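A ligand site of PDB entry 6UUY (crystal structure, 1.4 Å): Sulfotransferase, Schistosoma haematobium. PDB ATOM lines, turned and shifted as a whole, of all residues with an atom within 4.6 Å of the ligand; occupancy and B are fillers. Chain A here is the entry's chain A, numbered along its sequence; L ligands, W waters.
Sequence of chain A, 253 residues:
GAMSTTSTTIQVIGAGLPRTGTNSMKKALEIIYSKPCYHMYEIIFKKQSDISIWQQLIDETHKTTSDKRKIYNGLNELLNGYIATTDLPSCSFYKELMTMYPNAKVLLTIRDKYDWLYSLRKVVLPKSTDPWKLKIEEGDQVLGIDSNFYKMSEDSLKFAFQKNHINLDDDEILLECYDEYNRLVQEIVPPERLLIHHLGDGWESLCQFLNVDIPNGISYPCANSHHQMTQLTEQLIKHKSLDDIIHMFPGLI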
ATOM      1  N   PRO A  18      -5.333 -20.828   2.700  1.00  0.00           N
ATOM      2  CA  PRO A  18      -4.705 -21.432   1.515  1.00  0.00           C
ATOM      3  C   PRO A  18      -5.586 -22.485   0.859  1.00  0.00           C
ATOM      4  O   PRO A  18      -6.365 -23.183   1.516  1.00  0.00           O
ATOM      5  CB  PRO A  18      -3.391 -22.022   2.047  1.00  0.00           C
ATOM      6  CG  PRO A  18      -3.476 -21.974   3.505  1.00  0.00           C
ATOM      7  CD  PRO A  18      -4.442 -20.899   3.879  1.00  0.00           C
ATOM      8  N   HIS A  39       1.456 -12.657  -0.494  1.00  0.00           N
ATOM      9  CA  HIS A  39       1.047 -14.048  -0.611  1.00  0.00           C
ATOM     10  C   HIS A  39       2.196 -14.897  -0.079  1.00  0.00           C
ATOM     11  O   HIS A  39       3.332 -14.426   0.006  1.00  0.00           O
ATOM     12  CB  HIS A  39       0.772 -14.418  -2.088  1.00  0.00           C
ATOM     13  CG  HIS A  39       0.111 -15.750  -2.280  1.00  0.00           C
ATOM     14  ND1 HIS A  39       0.837 -16.913  -2.476  1.00  0.00           N
ATOM     15  CD2 HIS A  39      -1.195 -16.105  -2.316  1.00  0.00           C
ATOM     16  CE1 HIS A  39      -0.007 -17.925  -2.613  1.00  0.00           C
ATOM     17  NE2 HIS A  39      -1.248 -17.455  -2.527  1.00  0.00           N
ATOM     18  N   MET A  40       1.901 -16.146   0.287  1.00  0.00           N
ATOM     19  CA  MET A  40       2.985 -17.032   0.712  1.00  0.00           C
ATOM     20  C   MET A  40       4.063 -17.129  -0.368  1.00  0.00           C
ATOM     21  O   MET A  40       5.247 -17.254  -0.045  1.00  0.00           O
ATOM     22  CB  MET A  40       2.462 -18.411   1.083  1.00  0.00           C
ATOM     23  CG  MET A  40       3.540 -19.328   1.694  1.00  0.00           C
ATOM     24  SD  MET A  40       4.044 -18.857   3.356  1.00  0.00           S
ATOM     25  CE  MET A  40       2.770 -19.695   4.321  1.00  0.00           C
ATOM     26  N   TYR A  41       3.675 -17.061  -1.639  1.00  0.00           N
ATOM     27  CA  TYR A  41       4.658 -17.166  -2.714  1.00  0.00           C
ATOM     28  C   TYR A  41       5.630 -15.987  -2.737  1.00  0.00           C
ATOM     29  O   TYR A  41       6.735 -16.118  -3.281  1.00  0.00           O
ATOM     30  CB  TYR A  41       3.966 -17.338  -4.070  1.00  0.00           C
ATOM     31  CG  TYR A  41       3.372 -18.729  -4.289  1.00  0.00           C
ATOM     32  CD1 TYR A  41       3.350 -19.672  -3.263  1.00  0.00           C
ATOM     33  CD2 TYR A  41       2.826 -19.087  -5.512  1.00  0.00           C
ATOM     34  CE1 TYR A  41       2.811 -20.927  -3.459  1.00  0.00           C
ATOM     35  CE2 TYR A  41       2.291 -20.337  -5.717  1.00  0.00           C
ATOM     36  CZ  TYR A  41       2.281 -21.260  -4.687  1.00  0.00           C
ATOM     37  OH  TYR A  41       1.743 -22.515  -4.883  1.00  0.00           O
ATOM     38  N   ILE A  44       8.270 -17.440  -0.378  1.00  0.00           N
ATOM     39  CA  ILE A  44       9.007 -18.583  -0.908  1.00  0.00           C
ATOM     40  C   ILE A  44       9.938 -18.150  -2.037  1.00  0.00           C
ATOM     41  O   ILE A  44      11.112 -18.517  -2.074  1.00  0.00           O
ATOM     42  CB  ILE A  44       8.035 -19.679  -1.384  1.00  0.00           C
ATOM     43  CG1 ILE A  44       7.279 -20.264  -0.189  1.00  0.00           C
ATOM     44  CG2 ILE A  44       8.783 -20.765  -2.145  1.00  0.00           C
ATOM     45  CD1 ILE A  44       6.119 -21.163  -0.581  1.00  0.00           C
ATOM     46  N   PHE A  45       9.418 -17.360  -2.962  1.00  0.00           N
ATOM     47  CA  PHE A  45      10.137 -17.107  -4.201  1.00  0.00           C
ATOM     48  C   PHE A  45      10.896 -15.784  -4.214  1.00  0.00           C
ATOM     49  O   PHE A  45      11.779 -15.622  -5.059  1.00  0.00           O
ATOM     50  CB  PHE A  45       9.187 -17.212  -5.402  1.00  0.00           C
ATOM     51  CG  PHE A  45       8.607 -18.599  -5.589  1.00  0.00           C
ATOM     52  CD1 PHE A  45       9.364 -19.607  -6.159  1.00  0.00           C
ATOM     53  CD2 PHE A  45       7.325 -18.901  -5.153  1.00  0.00           C
ATOM     54  CE1 PHE A  45       8.851 -20.891  -6.312  1.00  0.00           C
ATOM     55  CE2 PHE A  45       6.792 -20.172  -5.307  1.00  0.00           C
ATOM     56  CZ  PHE A  45       7.556 -21.171  -5.895  1.00  0.00           C
ATOM     57  N   ASP A  87      -3.569 -14.999   1.746  1.00  0.00           N
ATOM     58  CA  ASP A  87      -2.929 -16.261   2.125  1.00  0.00           C
ATOM     59  C   ASP A  87      -2.365 -16.245   3.538  1.00  0.00           C
ATOM     60  O   ASP A  87      -2.270 -15.196   4.175  1.00  0.00           O
ATOM     61  CB  ASP A  87      -1.801 -16.579   1.131  1.00  0.00           C
ATOM     62  CG  ASP A  87      -1.425 -18.029   1.084  1.00  0.00           C
ATOM     63  OD1 ASP A  87      -2.020 -18.882   1.797  1.00  0.00           O
ATOM     64  OD2 ASP A  87      -0.496 -18.313   0.302  1.00  0.00           O
ATOM     65  N   LEU A  88      -1.983 -17.419   4.036  1.00  0.00           N
ATOM     66  CA  LEU A  88      -1.121 -17.471   5.201  1.00  0.00           C
ATOM     67  C   LEU A  88       0.262 -16.930   4.812  1.00  0.00           C
ATOM     68  O   LEU A  88       0.660 -17.015   3.647  1.00  0.00           O
ATOM     69  CB  LEU A  88      -0.981 -18.910   5.699  1.00  0.00           C
ATOM     70  CG  LEU A  88      -2.175 -19.504   6.452  1.00  0.00           C
ATOM     71  CD1 LEU A  88      -1.953 -20.973   6.728  1.00  0.00           C
ATOM     72  CD2 LEU A  88      -2.417 -18.759   7.764  1.00  0.00           C
ATOM     73  N   VAL A 123      -1.145 -30.643  -1.631  1.00  0.00           N
ATOM     74  CA  VAL A 123      -0.230 -29.558  -1.992  1.00  0.00           C
ATOM     75  C   VAL A 123       0.563 -29.041  -0.786  1.00  0.00           C
ATOM     76  O   VAL A 123       1.780 -28.891  -0.860  1.00  0.00           O
ATOM     77  CB  VAL A 123      -0.962 -28.403  -2.706  1.00  0.00           C
ATOM     78  CG1 VAL A 123       0.035 -27.307  -3.075  1.00  0.00           C
ATOM     79  CG2 VAL A 123      -1.694 -28.910  -3.929  1.00  0.00           C
ATOM     80  N   VAL A 124      -0.130 -28.702   0.304  1.00  0.00           N
ATOM     81  CA  VAL A 124       0.553 -27.957   1.366  1.00  0.00           C
ATOM     82  C   VAL A 124       0.639 -28.666   2.717  1.00  0.00           C
ATOM     83  O   VAL A 124       1.550 -28.374   3.505  1.00  0.00           O
ATOM     84  CB  VAL A 124       0.000 -26.527   1.545  1.00  0.00           C
ATOM     85  CG1 VAL A 124       0.087 -25.753   0.241  1.00  0.00           C
ATOM     86  CG2 VAL A 124      -1.413 -26.565   2.065  1.00  0.00           C
ATOM     87  N   LEU A 125      -0.282 -29.566   3.015  1.00  0.00           N
ATOM     88  CA  LEU A 125      -0.344 -30.201   4.343  1.00  0.00           C
ATOM     89  C   LEU A 125      -0.757 -31.658   4.226  1.00  0.00           C
ATOM     90  O   LEU A 125      -1.808 -32.080   4.720  1.00  0.00           O
ATOM     91  CB  LEU A 125      -1.279 -29.426   5.271  1.00  0.00           C
ATOM     92  CG  LEU A 125      -1.225 -29.787   6.767  1.00  0.00           C
ATOM     93  CD1 LEU A 125       0.035 -29.249   7.421  1.00  0.00           C
ATOM     94  CD2 LEU A 125      -2.459 -29.283   7.476  1.00  0.00           C
ATOM     95  N   ASP A 140      10.641 -29.087  -2.313  1.00  0.00           N
ATOM     96  CA  ASP A 140      10.761 -27.789  -1.643  1.00  0.00           C
ATOM     97  C   ASP A 140      12.197 -27.477  -1.263  1.00  0.00           C
ATOM     98  O   ASP A 140      12.590 -26.305  -1.231  1.00  0.00           O
ATOM     99  CB  ASP A 140       9.874 -27.749  -0.405  1.00  0.00           C
ATOM    100  CG  ASP A 140       8.409 -27.527  -0.735  1.00  0.00           C
ATOM    101  OD1 ASP A 140       8.111 -27.237  -1.912  1.00  0.00           O
ATOM    102  OD2 ASP A 140       7.555 -27.632   0.176  1.00  0.00           O
ATOM    103  N   LEU A 143      13.996 -25.284  -3.526  1.00  0.00           N
ATOM    104  CA  LEU A 143      13.656 -23.871  -3.423  1.00  0.00           C
ATOM    105  C   LEU A 143      14.305 -23.178  -2.234  1.00  0.00           C
ATOM    106  O   LEU A 143      14.100 -21.970  -2.061  1.00  0.00           O
ATOM    107  CB  LEU A 143      12.131 -23.695  -3.333  1.00  0.00           C
ATOM    108  CG  LEU A 143      11.289 -24.375  -4.415  1.00  0.00           C
ATOM    109  CD1 LEU A 143       9.804 -24.231  -4.108  1.00  0.00           C
ATOM    110  CD2 LEU A 143      11.637 -23.812  -5.781  1.00  0.00           C
ATOM    111  N   ILE A 145      13.561 -24.084   0.881  1.00  0.00           N
ATOM    112  CA  ILE A 145      12.647 -24.227   2.000  1.00  0.00           C
ATOM    113  C   ILE A 145      13.187 -25.286   2.961  1.00  0.00           C
ATOM    114  O   ILE A 145      13.671 -26.337   2.541  1.00  0.00           O
ATOM    115  CB  ILE A 145      11.253 -24.628   1.482  1.00  0.00           C
ATOM    116  CG1 ILE A 145      10.586 -23.463   0.764  1.00  0.00           C
ATOM    117  CG2 ILE A 145      10.373 -25.150   2.610  1.00  0.00           C
ATOM    118  CD1 ILE A 145       9.196 -23.783   0.231  1.00  0.00           C
ATOM    119  N   PHE A 149      10.796 -22.770   7.586  1.00  0.00           N
ATOM    120  CA  PHE A 149       9.621 -22.367   6.822  1.00  0.00           C
ATOM    121  C   PHE A 149       8.390 -23.137   7.275  1.00  0.00           C
ATOM    122  O   PHE A 149       7.313 -22.545   7.470  1.00  0.00           O
ATOM    123  CB  PHE A 149       9.857 -22.561   5.326  1.00  0.00           C
ATOM    124  CG  PHE A 149       8.621 -22.368   4.511  1.00  0.00           C
ATOM    125  CD1 PHE A 149       8.231 -21.086   4.127  1.00  0.00           C
ATOM    126  CD2 PHE A 149       7.820 -23.440   4.155  1.00  0.00           C
ATOM    127  CE1 PHE A 149       7.072 -20.892   3.393  1.00  0.00           C
ATOM    128  CE2 PHE A 149       6.661 -23.246   3.421  1.00  0.00           C
ATOM    129  CZ  PHE A 149       6.293 -21.972   3.031  1.00  0.00           C
ATOM    130  N   TYR A 150       8.515 -24.459   7.418  1.00  0.00           N
ATOM    131  CA  TYR A 150       7.363 -25.278   7.782  1.00  0.00           C
ATOM    132  C   TYR A 150       6.860 -24.943   9.179  1.00  0.00           C
ATOM    133  O   TYR A 150       5.648 -24.953   9.436  1.00  0.00           O
ATOM    134  CB  TYR A 150       7.721 -26.756   7.689  1.00  0.00           C
ATOM    135  CG  TYR A 150       7.991 -27.232   6.276  1.00  0.00           C
ATOM    136  CD1 TYR A 150       7.078 -26.984   5.252  1.00  0.00           C
ATOM    137  CD2 TYR A 150       9.158 -27.909   5.966  1.00  0.00           C
ATOM    138  CE1 TYR A 150       7.333 -27.423   3.962  1.00  0.00           C
ATOM    139  CE2 TYR A 150       9.421 -28.343   4.681  1.00  0.00           C
ATOM    140  CZ  TYR A 150       8.505 -28.104   3.687  1.00  0.00           C
ATOM    141  OH  TYR A 150       8.764 -28.542   2.411  1.00  0.00           O
ATOM    142  N   SER A 153       4.869 -21.700   8.910  1.00  0.00           N
ATOM    143  CA  SER A 153       3.599 -21.910   8.218  1.00  0.00           C
ATOM    144  C   SER A 153       2.610 -22.648   9.103  1.00  0.00           C
ATOM    145  O   SER A 153       1.439 -22.240   9.198  1.00  0.00           O
ATOM    146  CB  SER A 153       3.846 -22.679   6.920  1.00  0.00           C
ATOM    147  OG  SER A 153       4.684 -21.923   6.078  1.00  0.00           O
ATOM    148  N   GLU A 154       3.038 -23.753   9.728  1.00  0.00           N
ATOM    149  CA  GLU A 154       2.180 -24.479  10.649  1.00  0.00           C
ATOM    150  C   GLU A 154       1.736 -23.582  11.799  1.00  0.00           C
ATOM    151  O   GLU A 154       0.565 -23.606  12.199  1.00  0.00           O
ATOM    152  CB  GLU A 154       2.915 -25.696  11.200  1.00  0.00           C
ATOM    153  CG  GLU A 154       3.038 -26.838  10.220  1.00  0.00           C
ATOM    154  CD  GLU A 154       3.477 -28.144  10.877  1.00  0.00           C
ATOM    155  OE1 GLU A 154       3.652 -28.186  12.121  1.00  0.00           O
ATOM    156  OE2 GLU A 154       3.642 -29.130  10.129  1.00  0.00           O
ATOM    157  N   LEU A 157      -0.989 -21.339  10.722  1.00  0.00           N
ATOM    158  CA  LEU A 157      -2.258 -22.054  10.562  1.00  0.00           C
ATOM    159  C   LEU A 157      -2.904 -22.291  11.913  1.00  0.00           C
ATOM    160  O   LEU A 157      -4.107 -22.086  12.081  1.00  0.00           O
ATOM    161  CB  LEU A 157      -2.037 -23.377   9.817  1.00  0.00           C
ATOM    162  CG  LEU A 157      -3.289 -24.208   9.556  1.00  0.00           C
ATOM    163  CD1 LEU A 157      -4.257 -23.469   8.633  1.00  0.00           C
ATOM    164  CD2 LEU A 157      -2.953 -25.584   8.976  1.00  0.00           C
ATOM    165  N   MET A 229       0.650 -28.000  -9.213  1.00  0.00           N
ATOM    166  CA  MET A 229       1.536 -28.108  -8.055  1.00  0.00           C
ATOM    167  C   MET A 229       2.186 -29.487  -7.974  1.00  0.00           C
ATOM    168  O   MET A 229       3.374 -29.595  -7.652  1.00  0.00           O
ATOM    169  CB  MET A 229       0.760 -27.797  -6.772  1.00  0.00           C
ATOM    170  CG  MET A 229       0.467 -26.318  -6.579  1.00  0.00           C
ATOM    171  SD  MET A 229       1.957 -25.291  -6.596  1.00  0.00           S
ATOM    172  CE  MET A 229       1.899 -24.706  -8.265  1.00  0.00           C
ATOM    173  N   LEU A 232       4.879 -29.468 -10.410  1.00  0.00           N
ATOM    174  CA  LEU A 232       6.006 -28.662  -9.936  1.00  0.00           C
ATOM    175  C   LEU A 232       6.898 -29.460  -8.992  1.00  0.00           C
ATOM    176  O   LEU A 232       8.118 -29.501  -9.164  1.00  0.00           O
ATOM    177  CB  LEU A 232       5.503 -27.374  -9.281  1.00  0.00           C
ATOM    178  CG  LEU A 232       6.601 -26.455  -8.724  1.00  0.00           C
ATOM    179  CD1 LEU A 232       7.582 -26.009  -9.801  1.00  0.00           C
ATOM    180  CD2 LEU A 232       5.971 -25.242  -8.041  1.00  0.00           C
ATOM    181  N   THR A 233       6.304 -30.122  -7.999  1.00  0.00           N
ATOM    182  CA  THR A 233       7.096 -30.992  -7.122  1.00  0.00           C
ATOM    183  C   THR A 233       7.855 -32.048  -7.922  1.00  0.00           C
ATOM    184  O   THR A 233       9.052 -32.269  -7.692  1.00  0.00           O
ATOM    185  CB  THR A 233       6.175 -31.648  -6.094  1.00  0.00           C
ATOM    186  OG1 THR A 233       5.664 -30.638  -5.226  1.00  0.00           O
ATOM    187  CG2 THR A 233       6.934 -32.706  -5.269  1.00  0.00           C
HETATM  188  N1  LIG L   1       4.749 -25.059   1.008  1.00  0.00           N
HETATM  189  C1  LIG L   1       1.425 -22.368   1.238  1.00  0.00           C
HETATM  190  C2  LIG L   1       0.551 -24.307   6.130  1.00  0.00           C
HETATM  191  C3  LIG L   1       0.954 -25.203   7.095  1.00  0.00           C
HETATM  192  C4  LIG L   1       2.044 -26.023   6.894  1.00  0.00           C
HETATM  193  C5  LIG L   1       2.754 -25.938   5.707  1.00  0.00           C
HETATM  194  C6  LIG L   1       2.837 -24.087   2.267  1.00  0.00           C
HETATM  195  C7  LIG L   1       2.367 -25.038   4.716  1.00  0.00           C
HETATM  196  C8  LIG L   1       5.487 -25.183  -0.277  1.00  0.00           C
HETATM  197  C9  LIG L   1       6.054 -25.058  -2.997  1.00  0.00           C
HETATM  198  C10 LIG L   1       5.521 -27.463  -4.647  1.00  0.00           C
HETATM  199  C11 LIG L   1       3.206 -25.000   3.426  1.00  0.00           C
HETATM  200  C12 LIG L   1       2.209 -22.433   0.124  1.00  0.00           C
HETATM  201  C13 LIG L   1       3.273 -23.281   0.019  1.00  0.00           C
HETATM  202  C14 LIG L   1       1.257 -24.222   4.929  1.00  0.00           C
HETATM  203  C15 LIG L   1       1.749 -23.190   2.292  1.00  0.00           C
HETATM  204  C16 LIG L   1       3.605 -24.123   1.078  1.00  0.00           C
HETATM  205  N2  LIG L   1       5.465 -26.291  -2.480  1.00  0.00           N
HETATM  206  C17 LIG L   1       0.234 -21.405   1.314  1.00  0.00           C
HETATM  207  O1  LIG L   1       4.320 -25.826   3.328  1.00  0.00           O
HETATM  208  C18 LIG L   1       4.670 -26.045  -1.252  1.00  0.00           C
HETATM  209  C19 LIG L   1       5.014 -24.119  -3.640  1.00  0.00           C
HETATM  210  C20 LIG L   1       4.652 -26.980  -3.483  1.00  0.00           C
HETATM  211  O2  LIG L   1      -0.007 -20.805   0.058  1.00  0.00           O
HETATM  212  S1  LIG L   1       0.665 -23.021   3.720  1.00  0.00           S
HETATM  213  O   HOH W   1      -0.884 -21.908  -2.321  1.00  0.00           O
HETATM  214  O   HOH W   2       7.769 -29.662  -3.699  1.00  0.00           O
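A ring nitrogen (NE2) of His 39 lies close to the side-chain carboxylate (OD2) of Asp 87 (3.1 Å). OD2 of Asp 140 sits at hydrogen-bond distance from OH of Tyr 150, 2.7 Å away. SD of Met 229 is in hydrogen-bond range of OH of Tyr 41, at 3.3 Å. The side-chain carboxylate (OD2) of Asp 87 lies close to the backbone NH (N) of Met 40, at 3.2 Å. O of Asp 140 sits at hydrogen-bond distance from N of Ile 145, at 3.2 Å. The backbone carbonyl oxygen (O) of Phe 149 lies within hydrogen-bond range of the side-chain hydroxyl (OG) of Ser 153, 3.0 Å away. N of Tyr 41 sits at hydrogen-bond distance from ND1 of His 39 (3.0 Å). The side-chain hydroxyl (OG1) of Thr 233 lies within hydrogen-bond range of the backbone carbonyl oxygen (O) of Met 229 (3.5 Å).
OD1 of Asp 140 lies within salt-bridge range of N2 of the ligand, at 2.9 Å. The side-chain carboxylate (OD2) of Asp 87 lies within hydrogen-bond range of an oxygen (O2) of the ligand (2.6 Å).
Water W2 bridges the side-chain hydroxyl of Thr 233 and the side-chain carboxylate of Asp 140.
CB of Pro 18 touches C17 of the ligand, 3.7 Å away. His 39 touches the ligand (CE1 to O2, 3.9 Å). CB of Met 40 touches O2 of the ligand (3.6 Å). Tyr 41 touches the ligand (OH to C19, 3.8 Å). CD1 of Ile 44 touches C13 of the ligand, 3.6 Å away. O of Val 124 touches C5 of the ligand, 3.5 Å away. Leu 125 touches the ligand. Leu 143 touches the ligand (CD1 to C9, 3.998 Å). Ile 145 touches the ligand (CD1 to C8, 3.997 Å). Phe 149 touches the ligand (CE2 to O1, 3.5 Å). CE1 of Tyr 150 touches O1 of the ligand, 3.5 Å away. Ser 153 touches the ligand (CB to C7, 3.6 Å). Glu 154 touches the ligand. OG1 of Thr 233 touches C10 of the ligand, 3.2 Å away. Hydrophobic or aromatic side chains that line the ligand: Pro 18, His 39, Met 40, Tyr 41, Ile 44, Val 124, Leu 125, Leu 143, Ile 145, Phe 149 and Tyr 150. Within 4 Å of the ligand: Pro 18, His 39, Met 40, Tyr 41, Ile 44, Asp 87, Val 124, Leu 125, Asp 140, Leu 143, Ile 145, Phe 149, Tyr 150, Ser 153, Glu 154 and Thr 233. The nearest printed residue that does not touch the ligand is Val 123 (4.1 Å).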
